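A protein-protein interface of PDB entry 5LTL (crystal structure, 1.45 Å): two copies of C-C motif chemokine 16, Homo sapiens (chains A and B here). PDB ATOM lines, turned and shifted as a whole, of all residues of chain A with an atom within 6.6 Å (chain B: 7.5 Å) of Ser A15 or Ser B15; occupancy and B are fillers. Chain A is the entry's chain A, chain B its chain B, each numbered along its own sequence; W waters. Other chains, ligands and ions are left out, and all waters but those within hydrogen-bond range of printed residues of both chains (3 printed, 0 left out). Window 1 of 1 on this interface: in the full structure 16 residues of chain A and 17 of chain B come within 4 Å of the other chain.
Printed residues of chain B within 4 Å of Thr A13: Cys B56.
Of the printed residues of chain B, Pro A14 touches Thr B16 (3.6 Å), Cys B17 (3.6 Å), Ile B46 (3.7 Å) and Cys B56 (3.6 Å).
Cys A18 touches none of the printed residues of chain B.
Of the printed residues of chain A, Thr B13 touches Cys A56.
Ser B15 touches just these residues of chain A: Ser A15, Thr A16, Cys A17 and Leu A19.
Cys B18 touches none of the printed residues of chain A.
Of the printed residues of chain A, Leu B19 touches Ser A15 (3.9 Å) and Asn A39 (3.4 Å).
Of the printed residues of chain A, Asn B39 touches Leu A19.
The nearest residue of chain A that does not touch Ser B15 is Cys A18 (4.8 Å).
The nearest printed residue of chain A that does not touch Leu B19 is Cys A17 (4.2 Å).
Of the 15 printed residues of chain B, 10 touch a printed residue of chain A.
Along chain B the printed residues that touch a printed residue of chain A span positions 12 to 56.
Among the printed residues, 20 pairs touch across the chains.
Among the printed residues, no Asp or Glu carboxylate lies within 4 Å of a Lys or Arg side-chain nitrogen of the other chain.
Pro A14 touches Thr B16, and with the chains exchanged Thr A16 touches Pro B14.
Pro A14 touches Cys B56, and with the chains exchanged Cys A56 touches Pro B14.
Ser A15 touches Thr B16, and with the chains exchanged Thr A16 touches Ser B15.
Leu A19 touches Asn B39, and with the chains exchanged Asn A39 touches Leu B19.
Positions printed for both chains: 13, 14, 15, 16, 17, 18, 19, 39, 40, 46 and 56.
Of the 20 pairs that touch across the chains among the printed residues, 19 have their exchanged pair printed and touching as well.
The side-chain sulfur (SG) of Cys A17 is disulfide-bonded to the side-chain sulfur (SG) of Cys A40 (2.0 Å).
SG of Cys A56 is disulfide-bonded to SG of Cys A18 (2.0 Å).
SG of Cys B17 forms a disulfide with SG of Cys B40, 2.0 Å away.
The side-chain sulfur of Cys B18 is disulfide-bonded to the side-chain sulfur of Cys B56 (2.0 Å).
Among the printed residues, pairs that only touch across the chains: Asn A39 with Leu B19 (3.4 Å), Ser A15 with Thr B16 (3.4 Å), Thr A16 with Ser B15 (3.4 Å), Leu A19 with Ser B15 (3.4 Å), Thr A16 with Pro B14 (3.5 Å), Cys A17 with Pro B14 (3.6 Å), Pro A14 with Thr B16 (3.6 Å), Pro A14 with Cys B17 (3.6 Å), Ser A15 with Ser B15 (3.6 Å), Ile A46 with Pro B14 (3.7 Å), Leu A19 with Asn B39 (3.7 Å), Pro A14 with Ile B46 (3.7 Å), Cys A56 with Thr B13 (3.8 Å), Thr A13 with Cys B56 (3.8 Å) and Ser A15 with Leu B19 (3.9 Å).
Water W1 lies within hydrogen-bond range of the backbone carbonyl oxygen of Thr B13 (2.7 Å), the backbone NH of Leu A19 (2.8 Å) and the side-chain hydroxyl of Ser B15 (3.2 Å).
Water W3 lies within hydrogen-bond range of OG1 of Thr B16 (2.9 Å) and OG1 of Thr A16 (3.0 Å).
Water W2 lies within hydrogen-bond range of the backbone NH (N) of Leu B19, the backbone carbonyl oxygen (O) of Thr A13 and the side-chain sulfur (SG) of Cys B56.
N of Ser A15 lies within hydrogen-bond range of O of Cys B17 (2.6 Å).
O of Cys A17 sits at hydrogen-bond distance from N of Ser B15 (2.7 Å).
The backbone NH (N) of Cys A56 lies within hydrogen-bond range of the backbone carbonyl oxygen (O) of Asn B12, at 2.9 Å.
N of Pro A14 lies close to SG of Cys B56.
SG of Cys A56 sits close to N of Pro B14, at 3.5 Å.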
ATOM      1  N   THR A  13      -9.533  18.064  24.640  1.00  0.00           N
ATOM      2  CA  THR A  13      -8.693  18.370  23.488  1.00  0.00           C
ATOM      3  C   THR A  13      -7.922  19.662  23.740  1.00  0.00           C
ATOM      4  O   THR A  13      -8.456  20.592  24.342  1.00  0.00           O
ATOM      5  CB  THR A  13      -9.557  18.472  22.201  1.00  0.00           C
ATOM      6  OG1 THR A  13      -9.712  17.169  21.627  1.00  0.00           O
ATOM      7  CG2 THR A  13      -8.934  19.399  21.165  1.00  0.00           C
ATOM      8  N   PRO A  14      -6.654  19.716  23.302  1.00  0.00           N
ATOM      9  CA  PRO A  14      -5.838  20.927  23.442  1.00  0.00           C
ATOM     10  C   PRO A  14      -6.446  22.140  22.744  1.00  0.00           C
ATOM     11  O   PRO A  14      -7.203  21.997  21.782  1.00  0.00           O
ATOM     12  CB  PRO A  14      -4.527  20.548  22.747  1.00  0.00           C
ATOM     13  CG  PRO A  14      -4.476  19.081  22.791  1.00  0.00           C
ATOM     14  CD  PRO A  14      -5.887  18.600  22.721  1.00  0.00           C
ATOM     15  N   SER A  15      -6.095  23.326  23.228  1.00  0.00           N
ATOM     16  CA  SER A  15      -6.523  24.572  22.615  1.00  0.00           C
ATOM     17  C   SER A  15      -5.306  25.390  22.216  1.00  0.00           C
ATOM     18  O   SER A  15      -4.181  25.081  22.593  1.00  0.00           O
ATOM     19  CB  SER A  15      -7.370  25.401  23.591  1.00  0.00           C
ATOM     20  OG  SER A  15      -8.753  25.141  23.430  1.00  0.00           O
ATOM     21  N   THR A  16      -5.530  26.436  21.440  1.00  0.00           N
ATOM     22  CA  THR A  16      -4.467  27.381  21.168  1.00  0.00           C
ATOM     23  C   THR A  16      -4.678  28.565  22.089  1.00  0.00           C
ATOM     24  O   THR A  16      -5.736  29.199  22.051  1.00  0.00           O
ATOM     25  CB  THR A  16      -4.484  27.811  19.697  1.00  0.00           C
ATOM     26  OG1 THR A  16      -4.244  26.657  18.883  1.00  0.00           O
ATOM     27  CG2 THR A  16      -3.414  28.837  19.418  1.00  0.00           C
ATOM     28  N   CYS A  17      -3.689  28.842  22.937  1.00  0.00           N
ATOM     29  CA  CYS A  17      -3.806  29.942  23.904  1.00  0.00           C
ATOM     30  C   CYS A  17      -2.543  30.774  23.966  1.00  0.00           C
ATOM     31  O   CYS A  17      -1.444  30.282  23.720  1.00  0.00           O
ATOM     32  CB  CYS A  17      -4.080  29.389  25.299  1.00  0.00           C
ATOM     33  SG  CYS A  17      -5.738  28.715  25.522  1.00  0.00           S
ATOM     34  N   CYS A  18      -2.712  32.043  24.322  1.00  0.00           N
ATOM     35  CA  CYS A  18      -1.600  32.967  24.474  1.00  0.00           C
ATOM     36  C   CYS A  18      -1.174  33.097  25.926  1.00  0.00           C
ATOM     37  O   CYS A  18      -2.007  33.106  26.823  1.00  0.00           O
ATOM     38  CB  CYS A  18      -2.009  34.339  23.948  1.00  0.00           C
ATOM     39  SG  CYS A  18      -2.226  34.351  22.154  1.00  0.00           S
ATOM     40  N   LEU A  19       0.129  33.224  26.144  1.00  0.00           N
ATOM     41  CA  LEU A  19       0.666  33.313  27.492  1.00  0.00           C
ATOM     42  C   LEU A  19       1.084  34.740  27.830  1.00  0.00           C
ATOM     43  O   LEU A  19       1.291  35.059  28.999  1.00  0.00           O
ATOM     44  CB  LEU A  19       1.840  32.354  27.663  1.00  0.00           C
ATOM     45  CG  LEU A  19       1.515  30.891  27.348  1.00  0.00           C
ATOM     46  CD1 LEU A  19       2.794  30.080  27.371  1.00  0.00           C
ATOM     47  CD2 LEU A  19       0.489  30.339  28.320  1.00  0.00           C
ATOM     48  N   ASN A  39     -11.280  32.033  25.211  1.00  0.00           N
ATOM     49  CA  ASN A  39     -11.560  31.107  26.303  1.00  0.00           C
ATOM     50  C   ASN A  39     -10.285  30.479  26.841  1.00  0.00           C
ATOM     51  O   ASN A  39     -10.210  29.260  27.033  1.00  0.00           O
ATOM     52  CB  ASN A  39     -12.513  30.010  25.849  1.00  0.00           C
ATOM     53  CG  ASN A  39     -13.890  30.536  25.529  1.00  0.00           C
ATOM     54  OD1 ASN A  39     -14.577  31.074  26.397  1.00  0.00           O
ATOM     55  ND2 ASN A  39     -14.310  30.370  24.284  1.00  0.00           N
ATOM     56  N   CYS A  40      -9.283  31.312  27.059  1.00  0.00           N
ATOM     57  CA  CYS A  40      -8.019  30.932  27.661  1.00  0.00           C
ATOM     58  C   CYS A  40      -7.828  31.761  28.918  1.00  0.00           C
ATOM     59  O   CYS A  40      -8.504  32.780  29.101  1.00  0.00           O
ATOM     60  CB  CYS A  40      -6.878  31.238  26.690  1.00  0.00           C
ATOM     61  SG  CYS A  40      -6.966  30.307  25.144  1.00  0.00           S
ATOM     62  N   ILE A  46      -5.404  36.508  18.087  1.00  0.00           N
ATOM     63  CA  ILE A  46      -4.159  36.104  17.457  1.00  0.00           C
ATOM     64  C   ILE A  46      -4.162  36.590  16.008  1.00  0.00           C
ATOM     65  O   ILE A  46      -4.995  36.179  15.214  1.00  0.00           O
ATOM     66  CB  ILE A  46      -4.009  34.575  17.474  1.00  0.00           C
ATOM     67  CG1 ILE A  46      -3.964  34.048  18.915  1.00  0.00           C
ATOM     68  CG2 ILE A  46      -2.758  34.161  16.716  1.00  0.00           C
ATOM     69  CD1 ILE A  46      -4.068  32.523  19.025  1.00  0.00           C
ATOM     70  N   CYS A  56       0.092  37.164  19.421  1.00  0.00           N
ATOM     71  CA  CYS A  56      -0.898  37.325  20.481  1.00  0.00           C
ATOM     72  C   CYS A  56      -1.109  38.791  20.838  1.00  0.00           C
ATOM     73  O   CYS A  56      -0.141  39.511  21.068  1.00  0.00           O
ATOM     74  CB  CYS A  56      -0.422  36.598  21.734  1.00  0.00           C
ATOM     75  SG  CYS A  56      -0.333  34.827  21.580  1.00  0.00           S
ATOM     76  N   VAL B  11       7.011  33.433  24.616  1.00  0.00           N
ATOM     77  CA  VAL B  11       7.024  34.343  23.477  1.00  0.00           C
ATOM     78  C   VAL B  11       5.655  34.978  23.274  1.00  0.00           C
ATOM     79  O   VAL B  11       4.720  34.723  24.033  1.00  0.00           O
ATOM     80  CB  VAL B  11       7.434  33.619  22.180  1.00  0.00           C
ATOM     81  N   ASN B  12       5.546  35.808  22.242  1.00  0.00           N
ATOM     82  CA  ASN B  12       4.280  36.429  21.881  1.00  0.00           C
ATOM     83  C   ASN B  12       3.509  35.539  20.919  1.00  0.00           C
ATOM     84  O   ASN B  12       2.446  35.907  20.424  1.00  0.00           O
ATOM     85  CB  ASN B  12       4.521  37.796  21.251  1.00  0.00           C
ATOM     86  CG  ASN B  12       5.424  38.669  22.096  1.00  0.00           C
ATOM     87  OD1 ASN B  12       5.471  38.529  23.317  1.00  0.00           O
ATOM     88  ND2 ASN B  12       6.151  39.572  21.450  1.00  0.00           N
ATOM     89  N   THR B  13       4.069  34.367  20.651  1.00  0.00           N
ATOM     90  CA  THR B  13       3.417  33.383  19.804  1.00  0.00           C
ATOM     91  C   THR B  13       2.518  32.495  20.651  1.00  0.00           C
ATOM     92  O   THR B  13       2.846  32.176  21.796  1.00  0.00           O
ATOM     93  CB  THR B  13       4.445  32.527  19.036  1.00  0.00           C
ATOM     94  OG1 THR B  13       5.405  31.990  19.953  1.00  0.00           O
ATOM     95  CG2 THR B  13       5.170  33.375  18.012  1.00  0.00           C
ATOM     96  N   PRO B  14       1.370  32.090  20.098  1.00  0.00           N
ATOM     97  CA  PRO B  14       0.458  31.244  20.868  1.00  0.00           C
ATOM     98  C   PRO B  14       1.041  29.862  21.144  1.00  0.00           C
ATOM     99  O   PRO B  14       1.960  29.412  20.464  1.00  0.00           O
ATOM    100  CB  PRO B  14      -0.774  31.135  19.965  1.00  0.00           C
ATOM    101  CG  PRO B  14      -0.309  31.533  18.606  1.00  0.00           C
ATOM    102  CD  PRO B  14       0.792  32.513  18.814  1.00  0.00           C
ATOM    103  N   SER B  15       0.491  29.197  22.149  1.00  0.00           N
ATOM    104  CA  SER B  15       0.974  27.904  22.581  1.00  0.00           C
ATOM    105  C   SER B  15      -0.162  26.914  22.477  1.00  0.00           C
ATOM    106  O   SER B  15      -1.332  27.309  22.438  1.00  0.00           O
ATOM    107  CB  SER B  15       1.437  27.974  24.031  1.00  0.00           C
ATOM    108  OG  SER B  15       2.481  28.913  24.186  1.00  0.00           O
ATOM    109  N   THR B  16       0.173  25.633  22.427  1.00  0.00           N
ATOM    110  CA  THR B  16      -0.851  24.621  22.528  1.00  0.00           C
ATOM    111  C   THR B  16      -1.049  24.334  24.001  1.00  0.00           C
ATOM    112  O   THR B  16      -0.111  23.926  24.690  1.00  0.00           O
ATOM    113  CB  THR B  16      -0.448  23.355  21.796  1.00  0.00           C
ATOM    114  OG1 THR B  16      -0.222  23.682  20.421  1.00  0.00           O
ATOM    115  CG2 THR B  16      -1.555  22.327  21.897  1.00  0.00           C
ATOM    116  N   CYS B  17      -2.257  24.581  24.494  1.00  0.00           N
ATOM    117  CA  CYS B  17      -2.516  24.467  25.927  1.00  0.00           C
ATOM    118  C   CYS B  17      -3.801  23.716  26.216  1.00  0.00           C
ATOM    119  O   CYS B  17      -4.759  23.784  25.441  1.00  0.00           O
ATOM    120  CB  CYS B  17      -2.604  25.853  26.565  1.00  0.00           C
ATOM    121  SG  CYS B  17      -1.029  26.697  26.626  1.00  0.00           S
ATOM    122  N   CYS B  18      -3.821  23.031  27.355  1.00  0.00           N
ATOM    123  CA  CYS B  18      -5.005  22.308  27.789  1.00  0.00           C
ATOM    124  C   CYS B  18      -5.814  23.093  28.811  1.00  0.00           C
ATOM    125  O   CYS B  18      -5.257  23.826  29.631  1.00  0.00           O
ATOM    126  CB  CYS B  18      -4.605  20.953  28.372  1.00  0.00           C
ATOM    127  SG  CYS B  18      -3.815  19.852  27.181  1.00  0.00           S
ATOM    128  N   LEU B  19      -7.133  22.933  28.757  1.00  0.00           N
ATOM    129  CA  LEU B  19      -8.032  23.608  29.685  1.00  0.00           C
ATOM    130  C   LEU B  19      -8.610  22.635  30.720  1.00  0.00           C
ATOM    131  O   LEU B  19      -9.060  23.049  31.787  1.00  0.00           O
ATOM    132  CB  LEU B  19      -9.149  24.325  28.919  1.00  0.00           C
ATOM    133  CG  LEU B  19      -8.691  25.284  27.813  1.00  0.00           C
ATOM    134  CD1 LEU B  19      -9.878  25.923  27.100  1.00  0.00           C
ATOM    135  CD2 LEU B  19      -7.768  26.358  28.375  1.00  0.00           C
ATOM    136  N   ALA B  37       2.956  20.212  27.147  1.00  0.00           N
ATOM    137  CA  ALA B  37       2.266  21.503  27.242  1.00  0.00           C
ATOM    138  C   ALA B  37       2.330  21.980  28.691  1.00  0.00           C
ATOM    139  O   ALA B  37       1.312  22.247  29.330  1.00  0.00           O
ATOM    140  CB  ALA B  37       0.835  21.353  26.772  1.00  0.00           C
ATOM    141  N   ASN B  39       4.056  24.620  29.987  1.00  0.00           N
ATOM    142  CA  ASN B  39       4.204  26.055  30.250  1.00  0.00           C
ATOM    143  C   ASN B  39       2.882  26.834  30.293  1.00  0.00           C
ATOM    144  O   ASN B  39       2.871  28.054  30.464  1.00  0.00           O
ATOM    145  CB  ASN B  39       5.170  26.689  29.247  1.00  0.00           C
ATOM    146  CG  ASN B  39       6.595  26.198  29.423  1.00  0.00           C
ATOM    147  OD1 ASN B  39       7.052  25.970  30.543  1.00  0.00           O
ATOM    148  ND2 ASN B  39       7.302  26.029  28.313  1.00  0.00           N
ATOM    149  N   CYS B  40       1.775  26.115  30.145  1.00  0.00           N
ATOM    150  CA  CYS B  40       0.442  26.711  30.165  1.00  0.00           C
ATOM    151  C   CYS B  40      -0.078  26.863  31.593  1.00  0.00           C
ATOM    152  O   CYS B  40       0.484  26.286  32.528  1.00  0.00           O
ATOM    153  CB  CYS B  40      -0.522  25.835  29.362  1.00  0.00           C
ATOM    154  SG  CYS B  40       0.085  25.385  27.717  1.00  0.00           S
ATOM    155  N   ILE B  46       0.075  15.951  26.526  1.00  0.00           N
ATOM    156  CA  ILE B  46      -0.927  15.630  25.522  1.00  0.00           C
ATOM    157  C   ILE B  46      -0.538  14.318  24.871  1.00  0.00           C
ATOM    158  O   ILE B  46       0.538  14.217  24.292  1.00  0.00           O
ATOM    159  CB  ILE B  46      -0.978  16.712  24.432  1.00  0.00           C
ATOM    160  CG1 ILE B  46      -1.383  18.047  25.044  1.00  0.00           C
ATOM    161  CG2 ILE B  46      -1.957  16.315  23.329  1.00  0.00           C
ATOM    162  CD1 ILE B  46      -1.040  19.235  24.154  1.00  0.00           C
ATOM    163  N   CYS B  56      -5.583  15.645  26.585  1.00  0.00           N
ATOM    164  CA  CYS B  56      -4.922  16.365  27.667  1.00  0.00           C
ATOM    165  C   CYS B  56      -4.932  15.567  28.951  1.00  0.00           C
ATOM    166  O   CYS B  56      -5.987  15.089  29.376  1.00  0.00           O
ATOM    167  CB  CYS B  56      -5.627  17.699  27.927  1.00  0.00           C
ATOM    168  SG  CYS B  56      -5.511  18.893  26.575  1.00  0.00           S
ATOM    169  N   THR B  78       4.912  20.426  19.619  1.00  0.00           N
ATOM    170  CA  THR B  78       3.561  20.999  19.654  1.00  0.00           C
ATOM    171  C   THR B  78       3.288  21.861  18.425  1.00  0.00           C
ATOM    172  O   THR B  78       2.214  21.784  17.828  1.00  0.00           O
ATOM    173  CB  THR B  78       3.292  21.829  20.928  1.00  0.00           C
ATOM    174  OG1 THR B  78       4.481  22.531  21.313  1.00  0.00           O
ATOM    175  CG2 THR B  78       2.842  20.930  22.070  1.00  0.00           C
HETATM  176  O   HOH W   1       1.781  32.001  24.221  1.00  0.00           O
HETATM  177  O   HOH W   2      -8.653  20.688  27.500  1.00  0.00           O
HETATM  178  O   HOH W   3      -1.347  25.947  18.911  1.00  0.00           O
